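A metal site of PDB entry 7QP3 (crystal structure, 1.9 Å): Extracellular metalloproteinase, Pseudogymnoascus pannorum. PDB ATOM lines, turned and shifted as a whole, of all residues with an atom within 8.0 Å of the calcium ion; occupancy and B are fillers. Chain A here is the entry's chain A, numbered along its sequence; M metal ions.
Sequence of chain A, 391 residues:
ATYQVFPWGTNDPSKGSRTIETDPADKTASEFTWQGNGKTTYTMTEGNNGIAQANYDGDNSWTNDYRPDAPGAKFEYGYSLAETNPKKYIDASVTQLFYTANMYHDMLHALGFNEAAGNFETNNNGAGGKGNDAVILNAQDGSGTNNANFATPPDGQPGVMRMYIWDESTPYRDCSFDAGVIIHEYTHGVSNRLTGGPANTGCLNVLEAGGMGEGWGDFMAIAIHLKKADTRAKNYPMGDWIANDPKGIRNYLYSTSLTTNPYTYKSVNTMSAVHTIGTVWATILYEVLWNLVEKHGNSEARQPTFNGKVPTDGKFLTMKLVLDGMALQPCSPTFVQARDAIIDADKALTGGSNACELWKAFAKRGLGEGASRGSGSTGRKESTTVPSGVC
The side-chain hydroxyl (OG1) of Thr 195 lies within hydrogen-bond range of the backbone carbonyl oxygen (O) of Ser 191 (2.8 Å).
The side-chain amide oxygen of Asn 200 sits close to the backbone carbonyl oxygen of Gly 196, at 3.2 Å.
The guanidinium group (NH2) of Arg 193 sits at hydrogen-bond distance from the backbone carbonyl oxygen (O) of Pro 154, at 3.3 Å.
NH1 of Arg 193 lies close to OD1 of Asp 155 (3.2 Å).
The backbone carbonyl oxygen (O) of Pro 153 lies within hydrogen-bond range of the guanidinium group (NE) of Arg 193.
The guanidinium group (NH1) of Arg 193 lies within hydrogen-bond range of the backbone carbonyl oxygen (O) of Gly 118.
The backbone carbonyl oxygen of Pro 198 sits at hydrogen-bond distance from the backbone NH of Asp 155, 2.9 Å away.
SG of Cys 203 forms a disulfide with SG of Cys 331 (2.1 Å).
The calcium ion is bound by O of Gly 197 (2.2 Å), O of Thr 195 (2.3 Å), O of Asn 200 (2.3 Å), O of Asn 192 (2.4 Å) and O of Arg 193 (2.4 Å).
Merely in contact with the calcium ion: Gly 196 (3.8 Å), Leu 194 (3.9 Å) and Pro 198 (3.97 Å).
Within 4 Å of the calcium ion: Asn 192, Arg 193, Leu 194, Thr 195, Gly 196, Gly 197, Pro 198 and Asn 200.
The nearest printed residue that does not touch the calcium ion is Thr 201 (4.4 Å).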
ATOM      1  N   ALA A 117      27.213  -8.837  20.234  1.00  0.00           N
ATOM      2  CA  ALA A 117      26.117  -9.784  20.420  1.00  0.00           C
ATOM      3  C   ALA A 117      24.886  -9.176  21.098  1.00  0.00           C
ATOM      4  O   ALA A 117      23.828  -9.817  21.126  1.00  0.00           O
ATOM      5  CB  ALA A 117      26.593 -10.980  21.234  1.00  0.00           C
ATOM      6  N   GLY A 118      25.033  -7.971  21.631  1.00  0.00           N
ATOM      7  CA  GLY A 118      23.947  -7.278  22.285  1.00  0.00           C
ATOM      8  C   GLY A 118      24.024  -7.264  23.788  1.00  0.00           C
ATOM      9  O   GLY A 118      22.976  -7.301  24.424  1.00  0.00           O
ATOM     10  N   THR A 152      14.178  -6.350  29.936  1.00  0.00           N
ATOM     11  CA  THR A 152      15.147  -6.310  28.844  1.00  0.00           C
ATOM     12  C   THR A 152      14.610  -5.519  27.666  1.00  0.00           C
ATOM     13  O   THR A 152      13.827  -6.060  26.855  1.00  0.00           O
ATOM     14  CB  THR A 152      15.559  -7.708  28.353  1.00  0.00           C
ATOM     15  OG1 THR A 152      15.904  -8.522  29.463  1.00  0.00           O
ATOM     16  CG2 THR A 152      16.774  -7.591  27.450  1.00  0.00           C
ATOM     17  N   PRO A 153      15.031  -4.285  27.496  1.00  0.00           N
ATOM     18  CA  PRO A 153      14.722  -3.565  26.277  1.00  0.00           C
ATOM     19  C   PRO A 153      15.740  -3.891  25.191  1.00  0.00           C
ATOM     20  O   PRO A 153      16.762  -4.546  25.467  1.00  0.00           O
ATOM     21  CB  PRO A 153      14.811  -2.101  26.706  1.00  0.00           C
ATOM     22  CG  PRO A 153      15.899  -2.116  27.717  1.00  0.00           C
ATOM     23  CD  PRO A 153      15.867  -3.487  28.398  1.00  0.00           C
ATOM     24  N   PRO A 154      15.518  -3.425  23.973  1.00  0.00           N
ATOM     25  CA  PRO A 154      16.482  -3.674  22.894  1.00  0.00           C
ATOM     26  C   PRO A 154      17.853  -3.088  23.209  1.00  0.00           C
ATOM     27  O   PRO A 154      18.008  -2.221  24.063  1.00  0.00           O
ATOM     28  CB  PRO A 154      15.848  -2.997  21.679  1.00  0.00           C
ATOM     29  CG  PRO A 154      14.371  -3.030  21.965  1.00  0.00           C
ATOM     30  CD  PRO A 154      14.252  -2.854  23.481  1.00  0.00           C
ATOM     31  N   ASP A 155      18.852  -3.602  22.496  1.00  0.00           N
ATOM     32  CA  ASP A 155      20.224  -3.150  22.668  1.00  0.00           C
ATOM     33  C   ASP A 155      20.286  -1.626  22.596  1.00  0.00           C
ATOM     34  O   ASP A 155      19.605  -1.004  21.776  1.00  0.00           O
ATOM     35  CB  ASP A 155      21.110  -3.768  21.592  1.00  0.00           C
ATOM     36  CG  ASP A 155      22.582  -3.787  21.949  1.00  0.00           C
ATOM     37  OD1 ASP A 155      22.908  -3.683  23.159  1.00  0.00           O
ATOM     38  OD2 ASP A 155      23.400  -3.896  21.006  1.00  0.00           O
ATOM     39  N   GLY A 189      18.055 -11.198  30.565  1.00  0.00           N
ATOM     40  CA  GLY A 189      18.649 -10.247  29.635  1.00  0.00           C
ATOM     41  C   GLY A 189      19.351 -10.945  28.481  1.00  0.00           C
ATOM     42  O   GLY A 189      19.213 -10.556  27.319  1.00  0.00           O
ATOM     43  N   VAL A 190      20.127 -11.988  28.791  1.00  0.00           N
ATOM     44  CA  VAL A 190      20.953 -12.629  27.770  1.00  0.00           C
ATOM     45  C   VAL A 190      20.065 -13.273  26.708  1.00  0.00           C
ATOM     46  O   VAL A 190      20.317 -13.151  25.508  1.00  0.00           O
ATOM     47  CB  VAL A 190      21.878 -13.664  28.418  1.00  0.00           C
ATOM     48  CG1 VAL A 190      22.652 -14.459  27.377  1.00  0.00           C
ATOM     49  CG2 VAL A 190      22.817 -13.017  29.424  1.00  0.00           C
ATOM     50  N   SER A 191      19.084 -14.069  27.159  1.00  0.00           N
ATOM     51  CA  SER A 191      18.304 -14.843  26.223  1.00  0.00           C
ATOM     52  C   SER A 191      17.356 -13.944  25.432  1.00  0.00           C
ATOM     53  O   SER A 191      17.123 -14.192  24.240  1.00  0.00           O
ATOM     54  CB  SER A 191      17.565 -15.961  26.972  1.00  0.00           C
ATOM     55  OG  SER A 191      16.643 -15.491  27.930  1.00  0.00           O
ATOM     56  N   ASN A 192      16.856 -12.874  26.047  1.00  0.00           N
ATOM     57  CA  ASN A 192      16.024 -11.949  25.263  1.00  0.00           C
ATOM     58  C   ASN A 192      16.838 -11.171  24.244  1.00  0.00           C
ATOM     59  O   ASN A 192      16.364 -10.913  23.135  1.00  0.00           O
ATOM     60  CB  ASN A 192      15.254 -10.994  26.163  1.00  0.00           C
ATOM     61  CG  ASN A 192      13.928 -11.595  26.641  1.00  0.00           C
ATOM     62  OD1 ASN A 192      13.120 -12.065  25.850  1.00  0.00           O
ATOM     63  ND2 ASN A 192      13.717 -11.611  27.944  1.00  0.00           N
ATOM     64  N   ARG A 193      18.064 -10.760  24.589  1.00  0.00           N
ATOM     65  CA  ARG A 193      18.912 -10.106  23.592  1.00  0.00           C
ATOM     66  C   ARG A 193      19.289 -11.061  22.466  1.00  0.00           C
ATOM     67  O   ARG A 193      19.123 -10.740  21.271  1.00  0.00           O
ATOM     68  CB  ARG A 193      20.171  -9.540  24.262  1.00  0.00           C
ATOM     69  CG  ARG A 193      19.932  -8.267  25.092  1.00  0.00           C
ATOM     70  CD  ARG A 193      19.739  -7.036  24.193  1.00  0.00           C
ATOM     71  NE  ARG A 193      19.313  -5.869  24.946  1.00  0.00           N
ATOM     72  CZ  ARG A 193      20.127  -5.026  25.571  1.00  0.00           C
ATOM     73  NH1 ARG A 193      21.441  -5.175  25.555  1.00  0.00           N
ATOM     74  NH2 ARG A 193      19.612  -4.019  26.257  1.00  0.00           N
ATOM     75  N   LEU A 194      19.781 -12.255  22.810  1.00  0.00           N
ATOM     76  CA  LEU A 194      20.267 -13.156  21.772  1.00  0.00           C
ATOM     77  C   LEU A 194      19.138 -13.705  20.898  1.00  0.00           C
ATOM     78  O   LEU A 194      19.295 -13.860  19.685  1.00  0.00           O
ATOM     79  CB  LEU A 194      21.045 -14.302  22.408  1.00  0.00           C
ATOM     80  CG  LEU A 194      22.403 -13.940  22.951  1.00  0.00           C
ATOM     81  CD1 LEU A 194      23.070 -15.171  23.531  1.00  0.00           C
ATOM     82  CD2 LEU A 194      23.262 -13.297  21.846  1.00  0.00           C
ATOM     83  N   THR A 195      17.997 -14.028  21.494  1.00  0.00           N
ATOM     84  CA  THR A 195      16.962 -14.671  20.696  1.00  0.00           C
ATOM     85  C   THR A 195      16.386 -13.652  19.731  1.00  0.00           C
ATOM     86  O   THR A 195      15.933 -12.589  20.150  1.00  0.00           O
ATOM     87  CB  THR A 195      15.875 -15.281  21.585  1.00  0.00           C
ATOM     88  OG1 THR A 195      16.467 -16.224  22.459  1.00  0.00           O
ATOM     89  CG2 THR A 195      14.829 -16.018  20.727  1.00  0.00           C
ATOM     90  N   GLY A 196      16.428 -13.958  18.431  1.00  0.00           N
ATOM     91  CA  GLY A 196      15.910 -13.042  17.438  1.00  0.00           C
ATOM     92  C   GLY A 196      16.741 -11.808  17.203  1.00  0.00           C
ATOM     93  O   GLY A 196      16.297 -10.898  16.494  1.00  0.00           O
ATOM     94  N   GLY A 197      17.917 -11.717  17.814  1.00  0.00           N
ATOM     95  CA  GLY A 197      18.813 -10.621  17.585  1.00  0.00           C
ATOM     96  C   GLY A 197      18.604  -9.546  18.618  1.00  0.00           C
ATOM     97  O   GLY A 197      17.513  -9.382  19.154  1.00  0.00           O
ATOM     98  N   PRO A 198      19.646  -8.748  18.843  1.00  0.00           N
ATOM     99  CA  PRO A 198      19.637  -7.801  19.964  1.00  0.00           C
ATOM    100  C   PRO A 198      18.660  -6.630  19.842  1.00  0.00           C
ATOM    101  O   PRO A 198      18.409  -5.962  20.841  1.00  0.00           O
ATOM    102  CB  PRO A 198      21.092  -7.303  19.992  1.00  0.00           C
ATOM    103  CG  PRO A 198      21.618  -7.534  18.626  1.00  0.00           C
ATOM    104  CD  PRO A 198      20.900  -8.708  18.080  1.00  0.00           C
ATOM    105  N   ALA A 199      18.109  -6.357  18.654  1.00  0.00           N
ATOM    106  CA  ALA A 199      17.117  -5.292  18.514  1.00  0.00           C
ATOM    107  C   ALA A 199      15.709  -5.715  18.912  1.00  0.00           C
ATOM    108  O   ALA A 199      14.845  -4.851  19.079  1.00  0.00           O
ATOM    109  CB  ALA A 199      17.061  -4.794  17.068  1.00  0.00           C
ATOM    110  N   ASN A 200      15.471  -7.011  19.095  1.00  0.00           N
ATOM    111  CA  ASN A 200      14.136  -7.568  19.290  1.00  0.00           C
ATOM    112  C   ASN A 200      14.137  -8.323  20.607  1.00  0.00           C
ATOM    113  O   ASN A 200      14.808  -9.347  20.730  1.00  0.00           O
ATOM    114  CB  ASN A 200      13.766  -8.487  18.129  1.00  0.00           C
ATOM    115  CG  ASN A 200      13.905  -7.801  16.802  1.00  0.00           C
ATOM    116  OD1 ASN A 200      14.824  -8.100  16.026  1.00  0.00           O
ATOM    117  ND2 ASN A 200      13.016  -6.867  16.533  1.00  0.00           N
ATOM    118  N   THR A 201      13.395  -7.826  21.592  1.00  0.00           N
ATOM    119  CA  THR A 201      13.363  -8.473  22.893  1.00  0.00           C
ATOM    120  C   THR A 201      11.957  -8.945  23.271  1.00  0.00           C
ATOM    121  O   THR A 201      11.678  -9.177  24.444  1.00  0.00           O
ATOM    122  CB  THR A 201      13.984  -7.557  23.971  1.00  0.00           C
ATOM    123  OG1 THR A 201      13.307  -6.301  24.032  1.00  0.00           O
ATOM    124  CG2 THR A 201      15.501  -7.286  23.654  1.00  0.00           C
ATOM    125  N   GLY A 202      11.092  -9.164  22.264  1.00  0.00           N
ATOM    126  CA  GLY A 202       9.772  -9.767  22.445  1.00  0.00           C
ATOM    127  C   GLY A 202       9.670 -11.152  21.818  1.00  0.00           C
ATOM    128  O   GLY A 202       8.627 -11.543  21.295  1.00  0.00           O
ATOM    129  N   CYS A 203      10.759 -11.918  21.875  1.00  0.00           N
ATOM    130  CA  CYS A 203      10.834 -13.230  21.246  1.00  0.00           C
ATOM    131  C   CYS A 203      10.627 -14.407  22.192  1.00  0.00           C
ATOM    132  O   CYS A 203      10.622 -15.548  21.731  1.00  0.00           O
ATOM    133  CB  CYS A 203      12.191 -13.388  20.542  1.00  0.00           C
ATOM    134  SG  CYS A 203      12.202 -12.433  18.996  1.00  0.00           S
ATOM    135  N   LEU A 204      10.430 -14.178  23.489  1.00  0.00           N
ATOM    136  CA  LEU A 204      10.302 -15.260  24.455  1.00  0.00           C
ATOM    137  C   LEU A 204       9.022 -15.130  25.257  1.00  0.00           C
ATOM    138  O   LEU A 204       8.979 -15.328  26.476  1.00  0.00           O
ATOM    139  CB  LEU A 204      11.522 -15.301  25.352  1.00  0.00           C
ATOM    140  CG  LEU A 204      12.798 -15.634  24.603  1.00  0.00           C
ATOM    141  CD1 LEU A 204      13.970 -15.483  25.537  1.00  0.00           C
ATOM    142  CD2 LEU A 204      12.714 -17.031  24.063  1.00  0.00           C
ATOM    143  N   MET A 326      21.058 -19.890  21.517  1.00  0.00           N
ATOM    144  CA  MET A 326      20.143 -18.759  21.623  1.00  0.00           C
ATOM    145  C   MET A 326      20.267 -17.845  20.413  1.00  0.00           C
ATOM    146  O   MET A 326      19.266 -17.322  19.920  1.00  0.00           O
ATOM    147  CB  MET A 326      20.405 -17.947  22.899  1.00  0.00           C
ATOM    148  CG  MET A 326      20.017 -18.640  24.187  1.00  0.00           C
ATOM    149  SD  MET A 326      20.732 -17.675  25.547  1.00  0.00           S
ATOM    150  CE  MET A 326      20.262 -18.726  26.923  1.00  0.00           C
ATOM    151  N   CYS A 331      12.878 -16.676  16.619  1.00  0.00           N
ATOM    152  CA  CYS A 331      11.985 -16.012  17.544  1.00  0.00           C
ATOM    153  C   CYS A 331      10.839 -16.961  17.921  1.00  0.00           C
ATOM    154  O   CYS A 331      10.424 -17.820  17.147  1.00  0.00           O
ATOM    155  CB  CYS A 331      11.467 -14.729  16.893  1.00  0.00           C
ATOM    156  SG  CYS A 331      10.695 -13.456  17.956  1.00  0.00           S
HETATM  157 CA    CA M   1      16.744 -10.595  20.828  1.00  0.00          CA
